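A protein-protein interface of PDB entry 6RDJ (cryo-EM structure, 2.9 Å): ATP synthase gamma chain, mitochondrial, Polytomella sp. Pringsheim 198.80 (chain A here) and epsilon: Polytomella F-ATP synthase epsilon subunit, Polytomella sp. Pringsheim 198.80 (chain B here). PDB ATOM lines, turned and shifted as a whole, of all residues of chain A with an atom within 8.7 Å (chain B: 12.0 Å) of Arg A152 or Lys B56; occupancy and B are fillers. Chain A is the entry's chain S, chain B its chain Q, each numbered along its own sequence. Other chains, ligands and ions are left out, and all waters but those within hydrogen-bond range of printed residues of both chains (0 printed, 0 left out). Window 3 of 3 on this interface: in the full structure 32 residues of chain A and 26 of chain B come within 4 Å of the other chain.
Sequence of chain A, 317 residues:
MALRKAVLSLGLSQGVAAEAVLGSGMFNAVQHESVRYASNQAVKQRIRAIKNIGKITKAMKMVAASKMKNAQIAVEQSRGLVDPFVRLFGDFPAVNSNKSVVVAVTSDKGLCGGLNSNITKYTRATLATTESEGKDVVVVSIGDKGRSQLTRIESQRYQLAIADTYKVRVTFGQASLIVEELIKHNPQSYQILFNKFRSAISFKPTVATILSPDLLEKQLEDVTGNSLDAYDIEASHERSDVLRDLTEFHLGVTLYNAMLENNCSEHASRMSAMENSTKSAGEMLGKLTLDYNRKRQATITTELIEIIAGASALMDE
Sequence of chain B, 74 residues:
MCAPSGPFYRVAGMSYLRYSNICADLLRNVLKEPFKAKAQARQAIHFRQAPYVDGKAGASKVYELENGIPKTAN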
ATOM      1  N   THR A 120     -27.762  27.445   4.433  1.00  0.00           N
ATOM      2  CA  THR A 120     -29.024  26.729   4.304  1.00  0.00           C
ATOM      3  C   THR A 120     -30.192  27.702   4.218  1.00  0.00           C
ATOM      4  O   THR A 120     -31.136  27.485   3.440  1.00  0.00           O
ATOM      5  CB  THR A 120     -29.198  25.764   5.471  1.00  0.00           C
ATOM      6  OG1 THR A 120     -28.015  24.973   5.594  1.00  0.00           O
ATOM      7  CG2 THR A 120     -30.353  24.828   5.214  1.00  0.00           C
ATOM      8  N   ARG A 124     -32.607  27.886   0.814  1.00  0.00           N
ATOM      9  CA  ARG A 124     -34.059  27.914   0.677  1.00  0.00           C
ATOM     10  C   ARG A 124     -34.562  29.276   0.214  1.00  0.00           C
ATOM     11  O   ARG A 124     -35.591  29.345  -0.461  1.00  0.00           O
ATOM     12  CB  ARG A 124     -34.740  27.493   1.977  1.00  0.00           C
ATOM     13  CG  ARG A 124     -34.359  28.294   3.184  1.00  0.00           C
ATOM     14  CD  ARG A 124     -34.844  27.592   4.436  1.00  0.00           C
ATOM     15  NE  ARG A 124     -36.282  27.727   4.621  1.00  0.00           N
ATOM     16  CZ  ARG A 124     -36.836  28.402   5.619  1.00  0.00           C
ATOM     17  NH1 ARG A 124     -36.071  28.995   6.523  1.00  0.00           N
ATOM     18  NH2 ARG A 124     -38.154  28.485   5.716  1.00  0.00           N
ATOM     19  N   LYS A 145     -22.185  18.734   6.642  1.00  0.00           N
ATOM     20  CA  LYS A 145     -23.109  19.626   7.321  1.00  0.00           C
ATOM     21  C   LYS A 145     -24.231  20.119   6.423  1.00  0.00           C
ATOM     22  O   LYS A 145     -25.034  20.949   6.858  1.00  0.00           O
ATOM     23  CB  LYS A 145     -22.353  20.815   7.905  1.00  0.00           C
ATOM     24  CG  LYS A 145     -21.366  20.440   8.982  1.00  0.00           C
ATOM     25  CD  LYS A 145     -22.055  19.710  10.108  1.00  0.00           C
ATOM     26  CE  LYS A 145     -21.049  19.042  11.019  1.00  0.00           C
ATOM     27  NZ  LYS A 145     -21.699  18.143  12.003  1.00  0.00           N
ATOM     28  N   GLY A 146     -24.311  19.637   5.189  1.00  0.00           N
ATOM     29  CA  GLY A 146     -25.410  19.974   4.314  1.00  0.00           C
ATOM     30  C   GLY A 146     -26.519  18.950   4.394  1.00  0.00           C
ATOM     31  O   GLY A 146     -27.694  19.316   4.440  1.00  0.00           O
ATOM     32  N   ARG A 147     -26.161  17.663   4.449  1.00  0.00           N
ATOM     33  CA  ARG A 147     -27.172  16.621   4.577  1.00  0.00           C
ATOM     34  C   ARG A 147     -27.817  16.611   5.953  1.00  0.00           C
ATOM     35  O   ARG A 147     -28.870  15.991   6.127  1.00  0.00           O
ATOM     36  CB  ARG A 147     -26.578  15.243   4.296  1.00  0.00           C
ATOM     37  CG  ARG A 147     -25.452  14.861   5.214  1.00  0.00           C
ATOM     38  CD  ARG A 147     -25.439  13.372   5.477  1.00  0.00           C
ATOM     39  NE  ARG A 147     -24.493  13.024   6.529  1.00  0.00           N
ATOM     40  CZ  ARG A 147     -24.768  13.079   7.828  1.00  0.00           C
ATOM     41  NH1 ARG A 147     -23.842  12.744   8.715  1.00  0.00           N
ATOM     42  NH2 ARG A 147     -25.962  13.472   8.247  1.00  0.00           N
ATOM     43  N   SER A 148     -27.208  17.274   6.927  1.00  0.00           N
ATOM     44  CA  SER A 148     -27.823  17.413   8.230  1.00  0.00           C
ATOM     45  C   SER A 148     -28.919  18.464   8.253  1.00  0.00           C
ATOM     46  O   SER A 148     -29.771  18.424   9.143  1.00  0.00           O
ATOM     47  CB  SER A 148     -26.759  17.765   9.267  1.00  0.00           C
ATOM     48  OG  SER A 148     -27.343  17.962  10.538  1.00  0.00           O
ATOM     49  N   GLN A 149     -28.920  19.402   7.314  1.00  0.00           N
ATOM     50  CA  GLN A 149     -29.864  20.510   7.358  1.00  0.00           C
ATOM     51  C   GLN A 149     -30.720  20.649   6.112  1.00  0.00           C
ATOM     52  O   GLN A 149     -31.857  21.117   6.214  1.00  0.00           O
ATOM     53  CB  GLN A 149     -29.129  21.836   7.595  1.00  0.00           C
ATOM     54  CG  GLN A 149     -28.242  21.827   8.808  1.00  0.00           C
ATOM     55  CD  GLN A 149     -27.409  23.066   8.928  1.00  0.00           C
ATOM     56  OE1 GLN A 149     -27.852  24.160   8.594  1.00  0.00           O
ATOM     57  NE2 GLN A 149     -26.183  22.903   9.404  1.00  0.00           N
ATOM     58  N   LEU A 150     -30.209  20.269   4.942  1.00  0.00           N
ATOM     59  CA  LEU A 150     -31.042  20.306   3.747  1.00  0.00           C
ATOM     60  C   LEU A 150     -32.108  19.227   3.792  1.00  0.00           C
ATOM     61  O   LEU A 150     -33.187  19.403   3.221  1.00  0.00           O
ATOM     62  CB  LEU A 150     -30.181  20.160   2.498  1.00  0.00           C
ATOM     63  CG  LEU A 150     -29.279  21.353   2.206  1.00  0.00           C
ATOM     64  CD1 LEU A 150     -28.418  21.049   1.027  1.00  0.00           C
ATOM     65  CD2 LEU A 150     -30.090  22.598   1.948  1.00  0.00           C
ATOM     66  N   THR A 151     -31.823  18.115   4.473  1.00  0.00           N
ATOM     67  CA  THR A 151     -32.863  17.155   4.821  1.00  0.00           C
ATOM     68  C   THR A 151     -33.915  17.787   5.727  1.00  0.00           C
ATOM     69  O   THR A 151     -35.114  17.525   5.579  1.00  0.00           O
ATOM     70  CB  THR A 151     -32.223  15.944   5.496  1.00  0.00           C
ATOM     71  OG1 THR A 151     -31.211  15.400   4.642  1.00  0.00           O
ATOM     72  CG2 THR A 151     -33.252  14.882   5.800  1.00  0.00           C
ATOM     73  N   ARG A 152     -33.489  18.651   6.651  1.00  0.00           N
ATOM     74  CA  ARG A 152     -34.441  19.327   7.526  1.00  0.00           C
ATOM     75  C   ARG A 152     -35.271  20.360   6.776  1.00  0.00           C
ATOM     76  O   ARG A 152     -36.390  20.670   7.198  1.00  0.00           O
ATOM     77  CB  ARG A 152     -33.720  19.998   8.697  1.00  0.00           C
ATOM     78  CG  ARG A 152     -33.010  19.048   9.639  1.00  0.00           C
ATOM     79  CD  ARG A 152     -33.916  18.578  10.761  1.00  0.00           C
ATOM     80  NE  ARG A 152     -34.789  17.484  10.349  1.00  0.00           N
ATOM     81  CZ  ARG A 152     -34.423  16.205  10.298  1.00  0.00           C
ATOM     82  NH1 ARG A 152     -35.292  15.282   9.909  1.00  0.00           N
ATOM     83  NH2 ARG A 152     -33.190  15.846  10.633  1.00  0.00           N
ATOM     84  N   ILE A 153     -34.754  20.910   5.685  1.00  0.00           N
ATOM     85  CA  ILE A 153     -35.515  21.859   4.876  1.00  0.00           C
ATOM     86  C   ILE A 153     -36.226  21.166   3.723  1.00  0.00           C
ATOM     87  O   ILE A 153     -37.455  21.138   3.671  1.00  0.00           O
ATOM     88  CB  ILE A 153     -34.608  23.001   4.370  1.00  0.00           C
ATOM     89  CG1 ILE A 153     -33.973  23.747   5.545  1.00  0.00           C
ATOM     90  CG2 ILE A 153     -35.411  23.969   3.531  1.00  0.00           C
ATOM     91  CD1 ILE A 153     -34.968  24.431   6.464  1.00  0.00           C
ATOM     92  N   GLU A 154     -35.474  20.580   2.797  1.00  0.00           N
ATOM     93  CA  GLU A 154     -36.023  19.983   1.580  1.00  0.00           C
ATOM     94  C   GLU A 154     -35.754  18.487   1.639  1.00  0.00           C
ATOM     95  O   GLU A 154     -34.765  18.012   1.086  1.00  0.00           O
ATOM     96  CB  GLU A 154     -35.394  20.600   0.347  1.00  0.00           C
ATOM     97  CG  GLU A 154     -35.467  22.107   0.294  1.00  0.00           C
ATOM     98  CD  GLU A 154     -36.862  22.609   0.009  1.00  0.00           C
ATOM     99  OE1 GLU A 154     -37.594  21.929  -0.738  1.00  0.00           O
ATOM    100  OE2 GLU A 154     -37.229  23.680   0.531  1.00  0.00           O
ATOM    101  N   SER A 155     -36.640  17.742   2.296  1.00  0.00           N
ATOM    102  CA  SER A 155     -36.372  16.329   2.535  1.00  0.00           C
ATOM    103  C   SER A 155     -36.621  15.487   1.296  1.00  0.00           C
ATOM    104  O   SER A 155     -35.968  14.455   1.106  1.00  0.00           O
ATOM    105  CB  SER A 155     -37.230  15.821   3.691  1.00  0.00           C
ATOM    106  OG  SER A 155     -36.853  14.505   4.064  1.00  0.00           O
ATOM    107  N   GLN A 156     -37.556  15.904   0.447  1.00  0.00           N
ATOM    108  CA  GLN A 156     -37.943  15.118  -0.716  1.00  0.00           C
ATOM    109  C   GLN A 156     -37.131  15.448  -1.955  1.00  0.00           C
ATOM    110  O   GLN A 156     -36.820  14.543  -2.736  1.00  0.00           O
ATOM    111  CB  GLN A 156     -39.428  15.323  -1.019  1.00  0.00           C
ATOM    112  CG  GLN A 156     -39.891  16.755  -0.877  1.00  0.00           C
ATOM    113  CD  GLN A 156     -41.398  16.874  -0.842  1.00  0.00           C
ATOM    114  OE1 GLN A 156     -42.090  15.965  -0.392  1.00  0.00           O
ATOM    115  NE2 GLN A 156     -41.915  17.999  -1.317  1.00  0.00           N
ATOM    116  N   TYR A 158     -34.054  16.589  -1.855  1.00  0.00           N
ATOM    117  CA  TYR A 158     -32.664  16.244  -1.599  1.00  0.00           C
ATOM    118  C   TYR A 158     -32.359  14.893  -2.217  1.00  0.00           C
ATOM    119  O   TYR A 158     -33.067  13.918  -1.964  1.00  0.00           O
ATOM    120  CB  TYR A 158     -32.386  16.207  -0.102  1.00  0.00           C
ATOM    121  CG  TYR A 158     -30.929  16.160   0.228  1.00  0.00           C
ATOM    122  CD1 TYR A 158     -30.302  14.958   0.492  1.00  0.00           C
ATOM    123  CD2 TYR A 158     -30.178  17.316   0.273  1.00  0.00           C
ATOM    124  CE1 TYR A 158     -28.968  14.906   0.788  1.00  0.00           C
ATOM    125  CE2 TYR A 158     -28.844  17.273   0.570  1.00  0.00           C
ATOM    126  CZ  TYR A 158     -28.247  16.064   0.824  1.00  0.00           C
ATOM    127  OH  TYR A 158     -26.917  16.010   1.123  1.00  0.00           O
ATOM    128  N   ALA A 161     -25.481  13.517  -1.775  1.00  0.00           N
ATOM    129  CA  ALA A 161     -24.698  13.986  -0.636  1.00  0.00           C
ATOM    130  C   ALA A 161     -23.229  13.697  -0.887  1.00  0.00           C
ATOM    131  O   ALA A 161     -22.785  12.565  -0.704  1.00  0.00           O
ATOM    132  CB  ALA A 161     -25.152  13.309   0.654  1.00  0.00           C
ATOM    133  N   ARG B  48     -16.308  11.259  -1.112  1.00  0.00           N
ATOM    134  CA  ARG B  48     -17.269  10.172  -1.070  1.00  0.00           C
ATOM    135  C   ARG B  48     -18.641  10.740  -1.390  1.00  0.00           C
ATOM    136  O   ARG B  48     -18.878  11.944  -1.266  1.00  0.00           O
ATOM    137  CB  ARG B  48     -17.266   9.471   0.292  1.00  0.00           C
ATOM    138  CG  ARG B  48     -18.058  10.180   1.359  1.00  0.00           C
ATOM    139  CD  ARG B  48     -18.278   9.298   2.559  1.00  0.00           C
ATOM    140  NE  ARG B  48     -19.479   9.696   3.279  1.00  0.00           N
ATOM    141  CZ  ARG B  48     -19.490  10.580   4.265  1.00  0.00           C
ATOM    142  NH1 ARG B  48     -20.629  10.892   4.863  1.00  0.00           N
ATOM    143  NH2 ARG B  48     -18.363  11.154   4.649  1.00  0.00           N
ATOM    144  N   GLN B  49     -19.549   9.870  -1.821  1.00  0.00           N
ATOM    145  CA  GLN B  49     -20.856  10.347  -2.242  1.00  0.00           C
ATOM    146  C   GLN B  49     -21.908   9.281  -1.998  1.00  0.00           C
ATOM    147  O   GLN B  49     -21.608   8.089  -1.900  1.00  0.00           O
ATOM    148  CB  GLN B  49     -20.860  10.760  -3.711  1.00  0.00           C
ATOM    149  CG  GLN B  49     -20.220   9.758  -4.631  1.00  0.00           C
ATOM    150  CD  GLN B  49     -20.783   9.845  -6.018  1.00  0.00           C
ATOM    151  OE1 GLN B  49     -21.933  10.230  -6.204  1.00  0.00           O
ATOM    152  NE2 GLN B  49     -19.980   9.486  -7.006  1.00  0.00           N
ATOM    153  N   ALA B  50     -23.153   9.732  -1.920  1.00  0.00           N
ATOM    154  CA  ALA B  50     -24.268   8.891  -1.524  1.00  0.00           C
ATOM    155  C   ALA B  50     -25.581   9.483  -2.013  1.00  0.00           C
ATOM    156  O   ALA B  50     -25.893  10.635  -1.690  1.00  0.00           O
ATOM    157  CB  ALA B  50     -24.293   8.741  -0.005  1.00  0.00           C
ATOM    158  N   PRO B  51     -26.375   8.747  -2.784  1.00  0.00           N
ATOM    159  CA  PRO B  51     -27.661   9.275  -3.238  1.00  0.00           C
ATOM    160  C   PRO B  51     -28.684   9.283  -2.117  1.00  0.00           C
ATOM    161  O   PRO B  51     -28.562   8.572  -1.123  1.00  0.00           O
ATOM    162  CB  PRO B  51     -28.076   8.305  -4.348  1.00  0.00           C
ATOM    163  CG  PRO B  51     -26.842   7.520  -4.672  1.00  0.00           C
ATOM    164  CD  PRO B  51     -26.073   7.454  -3.413  1.00  0.00           C
ATOM    165  N   TYR B  52     -29.711  10.112  -2.291  1.00  0.00           N
ATOM    166  CA  TYR B  52     -30.785  10.249  -1.306  1.00  0.00           C
ATOM    167  C   TYR B  52     -32.114  10.079  -2.032  1.00  0.00           C
ATOM    168  O   TYR B  52     -32.703  11.050  -2.510  1.00  0.00           O
ATOM    169  CB  TYR B  52     -30.703  11.582  -0.590  1.00  0.00           C
ATOM    170  CG  TYR B  52     -29.934  11.523   0.702  1.00  0.00           C
ATOM    171  CD1 TYR B  52     -30.559  11.766   1.915  1.00  0.00           C
ATOM    172  CD2 TYR B  52     -28.582  11.217   0.711  1.00  0.00           C
ATOM    173  CE1 TYR B  52     -29.854  11.709   3.102  1.00  0.00           C
ATOM    174  CE2 TYR B  52     -27.870  11.153   1.888  1.00  0.00           C
ATOM    175  CZ  TYR B  52     -28.510  11.401   3.080  1.00  0.00           C
ATOM    176  OH  TYR B  52     -27.805  11.346   4.255  1.00  0.00           O
ATOM    177  N   VAL B  53     -32.598   8.845  -2.089  1.00  0.00           N
ATOM    178  CA  VAL B  53     -33.781   8.549  -2.885  1.00  0.00           C
ATOM    179  C   VAL B  53     -35.072   8.748  -2.100  1.00  0.00           C
ATOM    180  O   VAL B  53     -36.121   9.007  -2.697  1.00  0.00           O
ATOM    181  CB  VAL B  53     -33.686   7.125  -3.456  1.00  0.00           C
ATOM    182  CG1 VAL B  53     -32.538   7.040  -4.444  1.00  0.00           C
ATOM    183  CG2 VAL B  53     -33.480   6.105  -2.342  1.00  0.00           C
ATOM    184  N   ASP B  54     -35.027   8.645  -0.774  1.00  0.00           N
ATOM    185  CA  ASP B  54     -36.229   8.750   0.035  1.00  0.00           C
ATOM    186  C   ASP B  54     -36.275   9.994   0.902  1.00  0.00           C
ATOM    187  O   ASP B  54     -37.363  10.534   1.121  1.00  0.00           O
ATOM    188  CB  ASP B  54     -36.373   7.511   0.935  1.00  0.00           C
ATOM    189  CG  ASP B  54     -35.215   7.351   1.904  1.00  0.00           C
ATOM    190  OD1 ASP B  54     -35.404   6.687   2.945  1.00  0.00           O
ATOM    191  OD2 ASP B  54     -34.122   7.891   1.632  1.00  0.00           O
ATOM    192  N   GLY B  55     -35.129  10.473   1.367  1.00  0.00           N
ATOM    193  CA  GLY B  55     -35.099  11.519   2.361  1.00  0.00           C
ATOM    194  C   GLY B  55     -34.082  11.255   3.448  1.00  0.00           C
ATOM    195  O   GLY B  55     -33.517  12.201   3.994  1.00  0.00           O
ATOM    196  N   LYS B  56     -33.825   9.990   3.780  1.00  0.00           N
ATOM    197  CA  LYS B  56     -32.825   9.703   4.804  1.00  0.00           C
ATOM    198  C   LYS B  56     -31.896   8.558   4.419  1.00  0.00           C
ATOM    199  O   LYS B  56     -30.786   8.460   4.946  1.00  0.00           O
ATOM    200  CB  LYS B  56     -33.494   9.393   6.148  1.00  0.00           C
ATOM    201  CG  LYS B  56     -33.986  10.622   6.906  1.00  0.00           C
ATOM    202  CD  LYS B  56     -32.921  11.211   7.818  1.00  0.00           C
ATOM    203  CE  LYS B  56     -33.528  11.665   9.146  1.00  0.00           C
ATOM    204  NZ  LYS B  56     -32.546  12.331  10.049  1.00  0.00           N
ATOM    205  N   ALA B  57     -32.337   7.679   3.527  1.00  0.00           N
ATOM    206  CA  ALA B  57     -31.528   6.517   3.201  1.00  0.00           C
ATOM    207  C   ALA B  57     -30.681   6.759   1.957  1.00  0.00           C
ATOM    208  O   ALA B  57     -30.909   7.692   1.182  1.00  0.00           O
ATOM    209  CB  ALA B  57     -32.411   5.286   2.992  1.00  0.00           C
ATOM    210  N   GLY B  58     -29.685   5.895   1.779  1.00  0.00           N
ATOM    211  CA  GLY B  58     -28.946   5.820   0.536  1.00  0.00           C
ATOM    212  C   GLY B  58     -27.676   5.004   0.641  1.00  0.00           C
ATOM    213  O   GLY B  58     -27.019   5.008   1.684  1.00  0.00           O
ATOM    214  N   ALA B  59     -27.313   4.311  -0.437  1.00  0.00           N
ATOM    215  CA  ALA B  59     -26.071   3.557  -0.486  1.00  0.00           C
ATOM    216  C   ALA B  59     -24.901   4.519  -0.647  1.00  0.00           C
ATOM    217  O   ALA B  59     -25.080   5.713  -0.868  1.00  0.00           O
ATOM    218  CB  ALA B  59     -26.106   2.541  -1.624  1.00  0.00           C
ATOM    219  N   SER B  60     -23.680   4.007  -0.568  1.00  0.00           N
ATOM    220  CA  SER B  60     -22.516   4.876  -0.548  1.00  0.00           C
ATOM    221  C   SER B  60     -21.612   4.594  -1.735  1.00  0.00           C
ATOM    222  O   SER B  60     -21.780   3.613  -2.461  1.00  0.00           O
ATOM    223  CB  SER B  60     -21.719   4.729   0.751  1.00  0.00           C
ATOM    224  OG  SER B  60     -20.395   5.198   0.578  1.00  0.00           O
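The backbone NH (N) of Ala A161 sits at hydrogen-bond distance from the backbone carbonyl oxygen (O) of Ala B50 (2.9 Å).
The backbone carbonyl oxygen of Tyr A158 sits close to the backbone carbonyl oxygen of Tyr B52 (2.9 Å).
OD2 of Asp B54 sits at hydrogen-bond distance from N of Lys B56 (3.0 Å).
O of Arg A147 sits at hydrogen-bond distance from OG1 of Thr A151.
CD of Arg A147 touches OH of Tyr B52, at 3.3 Å.
O of Gly B55 touches CG2 of Thr A151, at 3.2 Å.
Lys B56 touches Arg A152 (NZ to NH2, 3.6 Å).
O of Ser A155 touches CA of Gly B55 (3.3 Å).
O of Arg B48 touches O of Ala A161, 3.996 Å away.
Ala A161 touches Gln B49 (O to CA, 3.3 Å).
Ala A161 touches Tyr B52 (CB to CE2, 3.7 Å).
Of the printed residues of chain B, Arg A147 touches Tyr B52 (3.3 Å).
No residue of chain B comes within 4 Å of Ser A148.
No residue of chain B comes within 4 Å of Leu A150.
Of chain B, only Lys B56 comes within 4 Å of Arg A152.
No residue of chain B comes within 4 Å of Ile A153.
Printed residues of chain B within 4 Å of Tyr A158: Tyr B52 (2.9 Å).
Of the printed residues of chain B, Ala A161 touches Arg B48 (3.996 Å), Gln B49 (3.3 Å), Ala B50 (2.9 Å) and Tyr B52 (3.7 Å).
Printed residues of chain A within 4 Å of Ala B50: Ala A161.
Of the printed residues of chain A, Gly B55 touches Thr A151 (3.2 Å) and Ser A155 (3.3 Å).
Lys B56 touches one residue of chain A.
No residue of chain A comes within 4 Å of Ala B57.
The nearest printed residue of chain A that does not touch Arg B48 is Arg A147 (4.7 Å).
Of the 16 printed residues of chain A, 6 touch a printed residue of chain B.
Hydrophobic or aromatic side chains of chain A that line the printed part of chain B: Tyr A158 and Ala A161.
Along chain A the printed residues that touch a printed residue of chain B span positions 147 to 161.
Hydrophobic or aromatic side chains of chain B that line the printed part of chain A: Tyr B52.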
